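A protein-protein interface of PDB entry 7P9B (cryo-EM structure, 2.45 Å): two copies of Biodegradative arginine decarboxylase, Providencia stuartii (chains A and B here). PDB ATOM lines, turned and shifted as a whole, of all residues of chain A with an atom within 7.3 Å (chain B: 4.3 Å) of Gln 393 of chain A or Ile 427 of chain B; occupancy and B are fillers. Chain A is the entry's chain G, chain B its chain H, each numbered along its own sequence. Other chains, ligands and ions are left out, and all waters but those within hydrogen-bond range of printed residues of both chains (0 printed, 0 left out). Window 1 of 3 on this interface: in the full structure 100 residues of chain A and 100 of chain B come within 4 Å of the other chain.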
ATOM      1  N   TYR A 177      -2.200  10.476  14.457  1.00  0.00           N
ATOM      2  CA  TYR A 177      -2.571  11.886  14.530  1.00  0.00           C
ATOM      3  C   TYR A 177      -3.123  12.396  13.199  1.00  0.00           C
ATOM      4  O   TYR A 177      -4.180  13.039  13.153  1.00  0.00           O
ATOM      5  CB  TYR A 177      -1.341  12.684  14.954  1.00  0.00           C
ATOM      6  CG  TYR A 177      -1.522  14.167  14.956  1.00  0.00           C
ATOM      7  CD1 TYR A 177      -2.132  14.810  16.014  1.00  0.00           C
ATOM      8  CD2 TYR A 177      -1.096  14.927  13.886  1.00  0.00           C
ATOM      9  CE1 TYR A 177      -2.299  16.161  16.009  1.00  0.00           C
ATOM     10  CE2 TYR A 177      -1.265  16.274  13.875  1.00  0.00           C
ATOM     11  CZ  TYR A 177      -1.865  16.888  14.935  1.00  0.00           C
ATOM     12  OH  TYR A 177      -2.033  18.245  14.913  1.00  0.00           O
ATOM     13  N   PHE A 181      -7.039  13.775  12.511  1.00  0.00           N
ATOM     14  CA  PHE A 181      -7.465  15.115  12.131  1.00  0.00           C
ATOM     15  C   PHE A 181      -7.738  15.278  10.644  1.00  0.00           C
ATOM     16  O   PHE A 181      -8.318  16.290  10.252  1.00  0.00           O
ATOM     17  CB  PHE A 181      -6.448  16.153  12.589  1.00  0.00           C
ATOM     18  CG  PHE A 181      -6.543  16.474  14.044  1.00  0.00           C
ATOM     19  CD1 PHE A 181      -7.539  17.312  14.507  1.00  0.00           C
ATOM     20  CD2 PHE A 181      -5.649  15.947  14.948  1.00  0.00           C
ATOM     21  CE1 PHE A 181      -7.639  17.617  15.838  1.00  0.00           C
ATOM     22  CE2 PHE A 181      -5.743  16.250  16.284  1.00  0.00           C
ATOM     23  CZ  PHE A 181      -6.736  17.087  16.729  1.00  0.00           C
ATOM     24  N   SER A 225     -10.031  40.342  11.438  1.00  0.00           N
ATOM     25  CA  SER A 225     -10.081  38.963  11.884  1.00  0.00           C
ATOM     26  C   SER A 225      -8.885  38.686  12.784  1.00  0.00           C
ATOM     27  O   SER A 225      -7.754  39.039  12.448  1.00  0.00           O
ATOM     28  CB  SER A 225     -10.090  38.030  10.678  1.00  0.00           C
ATOM     29  OG  SER A 225     -10.144  36.677  11.060  1.00  0.00           O
ATOM     30  N   VAL A 226      -9.136  38.068  13.931  1.00  0.00           N
ATOM     31  CA  VAL A 226      -8.125  37.855  14.957  1.00  0.00           C
ATOM     32  C   VAL A 226      -8.060  36.371  15.275  1.00  0.00           C
ATOM     33  O   VAL A 226      -9.094  35.705  15.400  1.00  0.00           O
ATOM     34  CB  VAL A 226      -8.436  38.685  16.219  1.00  0.00           C
ATOM     35  CG1 VAL A 226      -7.520  38.312  17.353  1.00  0.00           C
ATOM     36  CG2 VAL A 226      -8.305  40.157  15.914  1.00  0.00           C
ATOM     37  N   VAL A 227      -6.840  35.853  15.398  1.00  0.00           N
ATOM     38  CA  VAL A 227      -6.588  34.449  15.686  1.00  0.00           C
ATOM     39  C   VAL A 227      -6.070  34.248  17.102  1.00  0.00           C
ATOM     40  O   VAL A 227      -5.581  33.168  17.428  1.00  0.00           O
ATOM     41  CB  VAL A 227      -5.624  33.834  14.660  1.00  0.00           C
ATOM     42  CG1 VAL A 227      -6.243  33.836  13.290  1.00  0.00           C
ATOM     43  CG2 VAL A 227      -4.323  34.590  14.640  1.00  0.00           C
ATOM     44  N   VAL A 228      -6.164  35.264  17.949  1.00  0.00           N
ATOM     45  CA  VAL A 228      -5.763  35.169  19.345  1.00  0.00           C
ATOM     46  C   VAL A 228      -6.968  35.392  20.262  1.00  0.00           C
ATOM     47  O   VAL A 228      -6.827  35.562  21.458  1.00  0.00           O
ATOM     48  CB  VAL A 228      -4.606  36.145  19.640  1.00  0.00           C
ATOM     49  CG1 VAL A 228      -4.030  35.952  21.033  1.00  0.00           C
ATOM     50  CG2 VAL A 228      -3.511  35.989  18.614  1.00  0.00           C
ATOM     51  N   GLY A 229      -8.162  35.375  19.698  1.00  0.00           N
ATOM     52  CA  GLY A 229      -9.366  35.511  20.485  1.00  0.00           C
ATOM     53  C   GLY A 229      -9.666  36.945  20.861  1.00  0.00           C
ATOM     54  O   GLY A 229      -8.992  37.894  20.469  1.00  0.00           O
ATOM     55  N   THR A 230     -10.732  37.095  21.638  1.00  0.00           N
ATOM     56  CA  THR A 230     -11.105  38.412  22.121  1.00  0.00           C
ATOM     57  C   THR A 230     -10.120  38.922  23.156  1.00  0.00           C
ATOM     58  O   THR A 230     -10.042  40.128  23.367  1.00  0.00           O
ATOM     59  CB  THR A 230     -12.527  38.375  22.673  1.00  0.00           C
ATOM     60  OG1 THR A 230     -13.393  37.917  21.642  1.00  0.00           O
ATOM     61  CG2 THR A 230     -13.002  39.747  23.082  1.00  0.00           C
ATOM     62  N   SER A 233      -8.036  40.676  20.759  1.00  0.00           N
ATOM     63  CA  SER A 233      -8.801  41.809  20.239  1.00  0.00           C
ATOM     64  C   SER A 233      -8.850  42.961  21.237  1.00  0.00           C
ATOM     65  O   SER A 233      -8.566  44.111  20.887  1.00  0.00           O
ATOM     66  CB  SER A 233     -10.217  41.370  19.876  1.00  0.00           C
ATOM     67  OG  SER A 233     -10.228  40.488  18.781  1.00  0.00           O
ATOM     68  N   SER A 383     -16.308  37.534  20.252  1.00  0.00           N
ATOM     69  CA  SER A 383     -15.660  36.233  20.367  1.00  0.00           C
ATOM     70  C   SER A 383     -16.480  35.276  19.521  1.00  0.00           C
ATOM     71  O   SER A 383     -17.485  34.724  19.961  1.00  0.00           O
ATOM     72  CB  SER A 383     -15.577  35.793  21.819  1.00  0.00           C
ATOM     73  OG  SER A 383     -14.917  34.557  21.928  1.00  0.00           O
ATOM     74  N   THR A 384     -16.044  35.092  18.281  1.00  0.00           N
ATOM     75  CA  THR A 384     -16.842  34.377  17.297  1.00  0.00           C
ATOM     76  C   THR A 384     -17.059  32.922  17.686  1.00  0.00           C
ATOM     77  O   THR A 384     -17.995  32.289  17.203  1.00  0.00           O
ATOM     78  CB  THR A 384     -16.156  34.483  15.938  1.00  0.00           C
ATOM     79  OG1 THR A 384     -15.823  35.851  15.698  1.00  0.00           O
ATOM     80  CG2 THR A 384     -17.084  34.074  14.857  1.00  0.00           C
ATOM     81  N   HIS A 385     -16.273  32.396  18.613  1.00  0.00           N
ATOM     82  CA  HIS A 385     -16.409  30.977  19.020  1.00  0.00           C
ATOM     83  C   HIS A 385     -17.355  30.813  20.207  1.00  0.00           C
ATOM     84  O   HIS A 385     -17.841  29.704  20.399  1.00  0.00           O
ATOM     85  CB  HIS A 385     -15.054  30.370  19.347  1.00  0.00           C
ATOM     86  CG  HIS A 385     -14.275  31.138  20.350  1.00  0.00           C
ATOM     87  ND1 HIS A 385     -14.470  30.985  21.703  1.00  0.00           N
ATOM     88  CD2 HIS A 385     -13.299  32.051  20.201  1.00  0.00           C
ATOM     89  CE1 HIS A 385     -13.658  31.785  22.345  1.00  0.00           C
ATOM     90  NE2 HIS A 385     -12.919  32.430  21.448  1.00  0.00           N
ATOM     91  N1  LLP A 386     -14.136  39.253  27.010  1.00  0.00           N
ATOM     92  C2  LLP A 386     -15.144  38.609  27.585  1.00  0.00           C
ATOM     93  C2' LLP A 386     -16.271  39.387  28.182  1.00  0.00           C
ATOM     94  C3  LLP A 386     -15.159  37.220  27.628  1.00  0.00           C
ATOM     95  O3  LLP A 386     -16.202  36.630  28.234  1.00  0.00           O
ATOM     96  C4  LLP A 386     -14.106  36.489  27.061  1.00  0.00           C
ATOM     97  C4' LLP A 386     -14.121  35.030  27.111  1.00  0.00           C
ATOM     98  C5  LLP A 386     -13.054  37.196  26.461  1.00  0.00           C
ATOM     99  C6  LLP A 386     -13.117  38.560  26.468  1.00  0.00           C
ATOM    100  C5' LLP A 386     -11.861  36.515  25.860  1.00  0.00           C
ATOM    101  OP4 LLP A 386     -12.190  35.818  24.624  1.00  0.00           O
ATOM    102  P   LLP A 386     -11.295  34.592  24.150  1.00  0.00           P
ATOM    103  OP1 LLP A 386     -11.829  33.412  24.904  1.00  0.00           O
ATOM    104  OP2 LLP A 386      -9.874  34.918  24.505  1.00  0.00           O
ATOM    105  OP3 LLP A 386     -11.520  34.513  22.676  1.00  0.00           O
ATOM    106  N   LLP A 386     -17.586  31.869  20.980  1.00  0.00           N
ATOM    107  CA  LLP A 386     -18.424  31.703  22.188  1.00  0.00           C
ATOM    108  CB  LLP A 386     -18.229  32.854  23.181  1.00  0.00           C
ATOM    109  CG  LLP A 386     -17.067  32.695  24.149  1.00  0.00           C
ATOM    110  CD  LLP A 386     -16.754  33.958  24.942  1.00  0.00           C
ATOM    111  CE  LLP A 386     -15.294  34.082  25.304  1.00  0.00           C
ATOM    112  NZ  LLP A 386     -15.122  34.343  26.730  1.00  0.00           N
ATOM    113  C   LLP A 386     -19.868  31.438  21.753  1.00  0.00           C
ATOM    114  O   LLP A 386     -20.370  30.358  22.068  1.00  0.00           O
ATOM    115  N   ALA A 390     -17.696  29.216  15.328  1.00  0.00           N
ATOM    116  CA  ALA A 390     -16.313  29.304  14.894  1.00  0.00           C
ATOM    117  C   ALA A 390     -15.438  28.513  15.849  1.00  0.00           C
ATOM    118  O   ALA A 390     -15.823  28.223  16.980  1.00  0.00           O
ATOM    119  CB  ALA A 390     -15.839  30.753  14.807  1.00  0.00           C
ATOM    120  N   LEU A 391     -14.253  28.158  15.371  1.00  0.00           N
ATOM    121  CA  LEU A 391     -13.271  27.500  16.209  1.00  0.00           C
ATOM    122  C   LEU A 391     -12.755  28.458  17.271  1.00  0.00           C
ATOM    123  O   LEU A 391     -12.840  29.678  17.136  1.00  0.00           O
ATOM    124  CB  LEU A 391     -12.103  26.990  15.372  1.00  0.00           C
ATOM    125  CG  LEU A 391     -12.368  25.868  14.376  1.00  0.00           C
ATOM    126  CD1 LEU A 391     -11.131  25.627  13.549  1.00  0.00           C
ATOM    127  CD2 LEU A 391     -12.782  24.614  15.096  1.00  0.00           C
ATOM    128  N   SER A 392     -12.212  27.886  18.340  1.00  0.00           N
ATOM    129  CA  SER A 392     -11.628  28.694  19.399  1.00  0.00           C
ATOM    130  C   SER A 392     -10.501  29.556  18.853  1.00  0.00           C
ATOM    131  O   SER A 392      -9.824  29.192  17.891  1.00  0.00           O
ATOM    132  CB  SER A 392     -11.108  27.812  20.529  1.00  0.00           C
ATOM    133  OG  SER A 392     -12.161  27.136  21.176  1.00  0.00           O
ATOM    134  N   GLN A 393     -10.311  30.704  19.490  1.00  0.00           N
ATOM    135  CA  GLN A 393      -9.348  31.760  19.211  1.00  0.00           C
ATOM    136  C   GLN A 393      -9.789  32.657  18.068  1.00  0.00           C
ATOM    137  O   GLN A 393      -9.108  33.629  17.797  1.00  0.00           O
ATOM    138  CB  GLN A 393      -7.939  31.248  18.883  1.00  0.00           C
ATOM    139  CG  GLN A 393      -7.334  30.376  19.929  1.00  0.00           C
ATOM    140  CD  GLN A 393      -5.903  30.063  19.643  1.00  0.00           C
ATOM    141  OE1 GLN A 393      -5.295  30.651  18.762  1.00  0.00           O
ATOM    142  NE2 GLN A 393      -5.372  29.086  20.338  1.00  0.00           N
ATOM    143  N   ALA A 394     -10.902  32.376  17.402  1.00  0.00           N
ATOM    144  CA  ALA A 394     -11.398  33.253  16.356  1.00  0.00           C
ATOM    145  C   ALA A 394     -12.105  34.445  16.981  1.00  0.00           C
ATOM    146  O   ALA A 394     -12.853  34.294  17.947  1.00  0.00           O
ATOM    147  CB  ALA A 394     -12.346  32.500  15.430  1.00  0.00           C
ATOM    148  N   SER A 395     -11.859  35.634  16.444  1.00  0.00           N
ATOM    149  CA  SER A 395     -12.487  36.822  16.995  1.00  0.00           C
ATOM    150  C   SER A 395     -12.558  37.904  15.929  1.00  0.00           C
ATOM    151  O   SER A 395     -11.836  37.869  14.936  1.00  0.00           O
ATOM    152  CB  SER A 395     -11.728  37.318  18.224  1.00  0.00           C
ATOM    153  OG  SER A 395     -12.338  38.460  18.782  1.00  0.00           O
ATOM    154  N   PHE A 396     -13.442  38.871  16.151  1.00  0.00           N
ATOM    155  CA  PHE A 396     -13.535  40.039  15.286  1.00  0.00           C
ATOM    156  C   PHE A 396     -13.392  41.324  16.078  1.00  0.00           C
ATOM    157  O   PHE A 396     -13.962  41.466  17.163  1.00  0.00           O
ATOM    158  CB  PHE A 396     -14.855  40.121  14.523  1.00  0.00           C
ATOM    159  CG  PHE A 396     -14.920  39.260  13.310  1.00  0.00           C
ATOM    160  CD1 PHE A 396     -14.195  39.588  12.185  1.00  0.00           C
ATOM    161  CD2 PHE A 396     -15.766  38.174  13.259  1.00  0.00           C
ATOM    162  CE1 PHE A 396     -14.267  38.815  11.060  1.00  0.00           C
ATOM    163  CE2 PHE A 396     -15.844  37.403  12.130  1.00  0.00           C
ATOM    164  CZ  PHE A 396     -15.094  37.726  11.031  1.00  0.00           C
ATOM    165  N   LEU A 424      -2.869  30.416  11.756  1.00  0.00           N
ATOM    166  CA  LEU A 424      -3.504  29.195  11.288  1.00  0.00           C
ATOM    167  C   LEU A 424      -4.758  29.559  10.507  1.00  0.00           C
ATOM    168  O   LEU A 424      -5.708  30.102  11.071  1.00  0.00           O
ATOM    169  CB  LEU A 424      -3.848  28.290  12.468  1.00  0.00           C
ATOM    170  CG  LEU A 424      -4.468  26.937  12.137  1.00  0.00           C
ATOM    171  CD1 LEU A 424      -3.496  26.071  11.367  1.00  0.00           C
ATOM    172  CD2 LEU A 424      -4.915  26.252  13.394  1.00  0.00           C
ATOM    173  N   ILE A 427      -8.570  28.917  11.506  1.00  0.00           N
ATOM    174  CA  ILE A 427      -9.270  29.865  12.369  1.00  0.00           C
ATOM    175  C   ILE A 427      -9.866  31.000  11.543  1.00  0.00           C
ATOM    176  O   ILE A 427     -11.003  31.437  11.772  1.00  0.00           O
ATOM    177  CB  ILE A 427      -8.312  30.393  13.451  1.00  0.00           C
ATOM    178  CG1 ILE A 427      -7.813  29.253  14.334  1.00  0.00           C
ATOM    179  CG2 ILE A 427      -8.979  31.451  14.290  1.00  0.00           C
ATOM    180  CD1 ILE A 427      -6.667  29.640  15.223  1.00  0.00           C
ATOM    181  N   SER A 430     -12.832  29.790   9.763  1.00  0.00           N
ATOM    182  CA  SER A 430     -13.988  29.670  10.642  1.00  0.00           C
ATOM    183  C   SER A 430     -14.633  31.027  10.899  1.00  0.00           C
ATOM    184  O   SER A 430     -15.859  31.123  10.956  1.00  0.00           O
ATOM    185  CB  SER A 430     -13.605  28.981  11.951  1.00  0.00           C
ATOM    186  OG  SER A 430     -12.749  29.780  12.731  1.00  0.00           O
ATOM    187  N   ASN A 431     -13.836  32.090  11.054  1.00  0.00           N
ATOM    188  CA  ASN A 431     -14.422  33.435  11.069  1.00  0.00           C
ATOM    189  C   ASN A 431     -15.228  33.710   9.809  1.00  0.00           C
ATOM    190  O   ASN A 431     -16.332  34.262   9.873  1.00  0.00           O
ATOM    191  CB  ASN A 431     -13.356  34.520  11.211  1.00  0.00           C
ATOM    192  CG  ASN A 431     -13.090  34.899  12.630  1.00  0.00           C
ATOM    193  OD1 ASN A 431     -13.989  34.899  13.456  1.00  0.00           O
ATOM    194  ND2 ASN A 431     -11.869  35.309  12.909  1.00  0.00           N
ATOM    195  N   VAL B 227       0.072  29.012  21.951  1.00  0.00           N
ATOM    196  CA  VAL B 227      -0.832  28.973  20.811  1.00  0.00           C
ATOM    197  C   VAL B 227      -0.846  30.292  20.056  1.00  0.00           C
ATOM    198  O   VAL B 227      -1.724  30.514  19.223  1.00  0.00           O
ATOM    199  CB  VAL B 227      -2.252  28.573  21.239  1.00  0.00           C
ATOM    200  CG1 VAL B 227      -2.264  27.172  21.783  1.00  0.00           C
ATOM    201  CG2 VAL B 227      -2.780  29.532  22.272  1.00  0.00           C
ATOM    202  N   SER B 392       0.410  25.833  12.424  1.00  0.00           N
ATOM    203  CA  SER B 392       0.813  27.210  12.656  1.00  0.00           C
ATOM    204  C   SER B 392       0.295  27.698  13.999  1.00  0.00           C
ATOM    205  O   SER B 392      -0.747  27.254  14.486  1.00  0.00           O
ATOM    206  CB  SER B 392       0.302  28.118  11.542  1.00  0.00           C
ATOM    207  OG  SER B 392       0.908  27.805  10.309  1.00  0.00           O
ATOM    208  N   GLN B 393       1.041  28.624  14.587  1.00  0.00           N
ATOM    209  CA  GLN B 393       0.848  29.276  15.875  1.00  0.00           C
ATOM    210  C   GLN B 393       1.304  28.409  17.035  1.00  0.00           C
ATOM    211  O   GLN B 393       1.273  28.879  18.158  1.00  0.00           O
ATOM    212  CB  GLN B 393      -0.601  29.697  16.150  1.00  0.00           C
ATOM    213  CG  GLN B 393      -1.197  30.593  15.119  1.00  0.00           C
ATOM    214  CD  GLN B 393      -2.533  31.116  15.532  1.00  0.00           C
ATOM    215  OE1 GLN B 393      -2.942  30.969  16.672  1.00  0.00           O
ATOM    216  NE2 GLN B 393      -3.255  31.671  14.588  1.00  0.00           N
ATOM    217  N   ALA B 394       1.734  27.175  16.805  1.00  0.00           N
ATOM    218  CA  ALA B 394       2.252  26.343  17.878  1.00  0.00           C
ATOM    219  C   ALA B 394       3.681  26.754  18.197  1.00  0.00           C
ATOM    220  O   ALA B 394       4.475  27.011  17.293  1.00  0.00           O
ATOM    221  CB  ALA B 394       2.196  24.871  17.489  1.00  0.00           C
ATOM    222  N   THR B 420      -4.521  33.577  25.201  1.00  0.00           N
ATOM    223  CA  THR B 420      -5.965  33.667  25.095  1.00  0.00           C
ATOM    224  C   THR B 420      -6.601  32.805  26.175  1.00  0.00           C
ATOM    225  O   THR B 420      -6.012  31.826  26.632  1.00  0.00           O
ATOM    226  CB  THR B 420      -6.444  33.236  23.699  1.00  0.00           C
ATOM    227  OG1 THR B 420      -7.861  33.373  23.608  1.00  0.00           O
ATOM    228  CG2 THR B 420      -6.048  31.810  23.399  1.00  0.00           C
ATOM    229  N   SER B 422      -9.295  31.130  25.597  1.00  0.00           N
ATOM    230  CA  SER B 422      -9.949  30.040  24.877  1.00  0.00           C
ATOM    231  C   SER B 422      -8.996  29.486  23.831  1.00  0.00           C
ATOM    232  O   SER B 422      -9.154  29.741  22.634  1.00  0.00           O
ATOM    233  CB  SER B 422     -11.242  30.521  24.220  1.00  0.00           C
ATOM    234  OG  SER B 422     -12.176  30.964  25.182  1.00  0.00           O
ATOM    235  N   PRO B 423      -7.992  28.719  24.244  1.00  0.00           N
ATOM    236  CA  PRO B 423      -7.061  28.156  23.266  1.00  0.00           C
ATOM    237  C   PRO B 423      -7.690  27.048  22.440  1.00  0.00           C
ATOM    238  O   PRO B 423      -8.537  26.287  22.907  1.00  0.00           O
ATOM    239  CB  PRO B 423      -5.921  27.623  24.136  1.00  0.00           C
ATOM    240  CG  PRO B 423      -6.526  27.392  25.442  1.00  0.00           C
ATOM    241  CD  PRO B 423      -7.574  28.429  25.623  1.00  0.00           C
ATOM    242  N   LEU B 424      -7.268  26.976  21.185  1.00  0.00           N
ATOM    243  CA  LEU B 424      -7.668  25.898  20.296  1.00  0.00           C
ATOM    244  C   LEU B 424      -6.799  24.680  20.573  1.00  0.00           C
ATOM    245  O   LEU B 424      -5.589  24.715  20.348  1.00  0.00           O
ATOM    246  CB  LEU B 424      -7.537  26.336  18.840  1.00  0.00           C
ATOM    247  CG  LEU B 424      -7.980  25.334  17.781  1.00  0.00           C
ATOM    248  CD1 LEU B 424      -9.464  25.062  17.880  1.00  0.00           C
ATOM    249  CD2 LEU B 424      -7.618  25.833  16.413  1.00  0.00           C
ATOM    250  N   TYR B 425      -7.416  23.604  21.055  1.00  0.00           N
ATOM    251  CA  TYR B 425      -6.651  22.449  21.502  1.00  0.00           C
ATOM    252  C   TYR B 425      -6.027  21.663  20.360  1.00  0.00           C
ATOM    253  O   TYR B 425      -5.183  20.805  20.615  1.00  0.00           O
ATOM    254  CB  TYR B 425      -7.527  21.528  22.347  1.00  0.00           C
ATOM    255  CG  TYR B 425      -7.798  22.070  23.721  1.00  0.00           C
ATOM    256  CD1 TYR B 425      -7.121  23.181  24.189  1.00  0.00           C
ATOM    257  CD2 TYR B 425      -8.697  21.449  24.567  1.00  0.00           C
ATOM    258  CE1 TYR B 425      -7.349  23.675  25.442  1.00  0.00           C
ATOM    259  CE2 TYR B 425      -8.931  21.936  25.827  1.00  0.00           C
ATOM    260  CZ  TYR B 425      -8.252  23.049  26.258  1.00  0.00           C
ATOM    261  OH  TYR B 425      -8.475  23.543  27.516  1.00  0.00           O
ATOM    262  N   ALA B 426      -6.410  21.932  19.115  1.00  0.00           N
ATOM    263  CA  ALA B 426      -5.719  21.305  17.994  1.00  0.00           C
ATOM    264  C   ALA B 426      -4.269  21.770  17.913  1.00  0.00           C
ATOM    265  O   ALA B 426      -3.371  20.981  17.605  1.00  0.00           O
ATOM    266  CB  ALA B 426      -6.464  21.601  16.695  1.00  0.00           C
ATOM    267  N   ILE B 427      -4.017  23.042  18.224  1.00  0.00           N
ATOM    268  CA  ILE B 427      -2.654  23.566  18.228  1.00  0.00           C
ATOM    269  C   ILE B 427      -1.837  22.920  19.342  1.00  0.00           C
ATOM    270  O   ILE B 427      -0.665  22.559  19.158  1.00  0.00           O
ATOM    271  CB  ILE B 427      -2.683  25.099  18.364  1.00  0.00           C
ATOM    272  CG1 ILE B 427      -3.412  25.732  17.182  1.00  0.00           C
ATOM    273  CG2 ILE B 427      -1.289  25.656  18.477  1.00  0.00           C
ATOM    274  CD1 ILE B 427      -3.729  27.186  17.381  1.00  0.00           C
ATOM    275  N   CYS B 428      -2.443  22.766  20.517  1.00  0.00           N
ATOM    276  CA  CYS B 428      -1.750  22.128  21.628  1.00  0.00           C
ATOM    277  C   CYS B 428      -1.455  20.667  21.318  1.00  0.00           C
ATOM    278  O   CYS B 428      -0.373  20.160  21.636  1.00  0.00           O
ATOM    279  CB  CYS B 428      -2.592  22.250  22.895  1.00  0.00           C
ATOM    280  SG  CYS B 428      -2.958  23.933  23.386  1.00  0.00           S
ATOM    281  N   ALA B 429      -2.407  19.980  20.693  1.00  0.00           N
ATOM    282  CA  ALA B 429      -2.193  18.597  20.294  1.00  0.00           C
ATOM    283  C   ALA B 429      -1.092  18.489  19.250  1.00  0.00           C
ATOM    284  O   ALA B 429      -0.350  17.503  19.226  1.00  0.00           O
ATOM    285  CB  ALA B 429      -3.495  18.001  19.771  1.00  0.00           C
ATOM    286  N   SER B 430      -0.962  19.492  18.382  1.00  0.00           N
ATOM    287  CA  SER B 430       0.123  19.457  17.409  1.00  0.00           C
ATOM    288  C   SER B 430       1.477  19.669  18.078  1.00  0.00           C
ATOM    289  O   SER B 430       2.457  19.028  17.698  1.00  0.00           O
ATOM    290  CB  SER B 430      -0.112  20.476  16.295  1.00  0.00           C
ATOM    291  OG  SER B 430      -0.012  21.798  16.769  1.00  0.00           O
ATOM    292  N   ASN B 431       1.559  20.557  19.076  1.00  0.00           N
ATOM    293  CA  ASN B 431       2.779  20.616  19.888  1.00  0.00           C
ATOM    294  C   ASN B 431       3.103  19.268  20.514  1.00  0.00           C
ATOM    295  O   ASN B 431       4.260  18.835  20.520  1.00  0.00           O
ATOM    296  CB  ASN B 431       2.672  21.656  21.002  1.00  0.00           C
ATOM    297  CG  ASN B 431       3.181  23.001  20.600  1.00  0.00           C
ATOM    298  OD1 ASN B 431       4.128  23.107  19.836  1.00  0.00           O
ATOM    299  ND2 ASN B 431       2.614  24.040  21.178  1.00  0.00           N
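Val 227 of chain A touches Gln 393 of chain B, and with the chains exchanged Gln 393 of chain A touches Val 227 of chain B. Ser 392 of chain A touches Leu 424 of chain B, and with the chains exchanged Leu 424 of chain A touches Ser 392 of chain B. Gln 393 of chain A touches its own counterpart, Gln 393 of chain B. Gln 393 of chain A touches Leu 424 of chain B, and with the chains exchanged Leu 424 of chain A touches Gln 393 of chain B. Of the 19 pairs that touch across the chains among the printed residues, 7 have their exchanged pair printed and touching as well.
Gln 393 of chain A touches seven residues of chain B. Of the printed residues of chain A, Ile 427 of chain B touches Gln 393 (3.9 Å). No residue of chain A comes within 4 Å of Ala 426 of chain B. Printed residues of chain A within 4 Å of Thr 420 of chain B: Val 228, LLP 386 and Gln 393. Of the printed residues of chain A, Ser 430 of chain B touches Tyr 177. Ser 395 of chain A touches none of the printed residues of chain B. The nearest residue of chain A that does not touch Ile 427 of chain B is Leu 424 of chain A (4.1 Å). The nearest printed residue of chain A that does not touch Val 227 of chain B is Val 227 of chain A (5.0 Å).
NE2 of His 385 of chain A is in hydrogen-bond range of OG of Ser 383 of chain A (3.0 Å). N of Ser 422 of chain B lies close to OG1 of Thr 420 of chain B (3.3 Å). The backbone NH of Val 228 of chain A is in hydrogen-bond range of the backbone carbonyl oxygen of Gln 393 of chain A, 3.4 Å away. O of Val 227 of chain A sits close to OE1 of Gln 393 of chain A, 2.9 Å away. N of Gly 229 of chain A lies within hydrogen-bond range of O of Gln 393 of chain A, 2.7 Å away. The backbone carbonyl oxygen of Val 227 of chain B sits close to the side-chain amide oxygen of Gln 393 of chain B, at 2.9 Å.
NE2 of Gln 393 of chain B lies close to N of Leu 424 of chain A (3.1 Å). OP1 of LLP 386 of chain A sits close to OG of Ser 422 of chain B (2.5 Å). The side-chain amide oxygen (OE1) of Gln 393 of chain A lies close to the side-chain amide oxygen (OE1) of Gln 393 of chain B (3.2 Å). N of Gln 393 of chain A lies close to O of Ser 422 of chain B, 3.5 Å away. The side-chain amide nitrogen of Gln 393 of chain A lies close to the backbone NH of Leu 424 of chain B. OG1 of Thr 420 of chain B is in hydrogen-bond range of O of Val 228 of chain A (3.2 Å). OP2 of LLP 386 of chain A sits close to OG1 of Thr 420 of chain B (2.7 Å).
Ala 429 of chain B touches Tyr 177 of chain A. CB of Ser 430 of chain B touches OH of Tyr 177 of chain A, at 3.3 Å. CE1 of His 385 of chain A touches OG of Ser 422 of chain B, at 3.3 Å. Ser 392 of chain A touches Ser 422 of chain B. Ser 392 of chain A touches Pro 423 of chain B (CB to O, 3.8 Å). Leu 424 of chain B touches Ser 392 of chain A (CB to O, 3.8 Å). Gln 393 of chain A touches Val 227 of chain B. Thr 420 of chain B touches Gln 393 of chain A (CG2 to CG, 3.97 Å). Pro 423 of chain B touches Gln 393 of chain A. Ser 392 of chain B touches Leu 424 of chain A (O to CB, 3.8 Å).
Hydrophobic or aromatic side chains of chain B within 4 Å of the printed part of chain A: Val 227, Leu 424 and Ile 427. Printed residues of chain A that touch a printed residue of chain B: Tyr 177, Val 227, Val 228, His 385, LLP 386, Ser 392, Gln 393 and Leu 424. Along chain A the printed residues that touch a printed residue of chain B span positions 177 to 424. Among the printed residues, 19 pairs touch across the chains.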
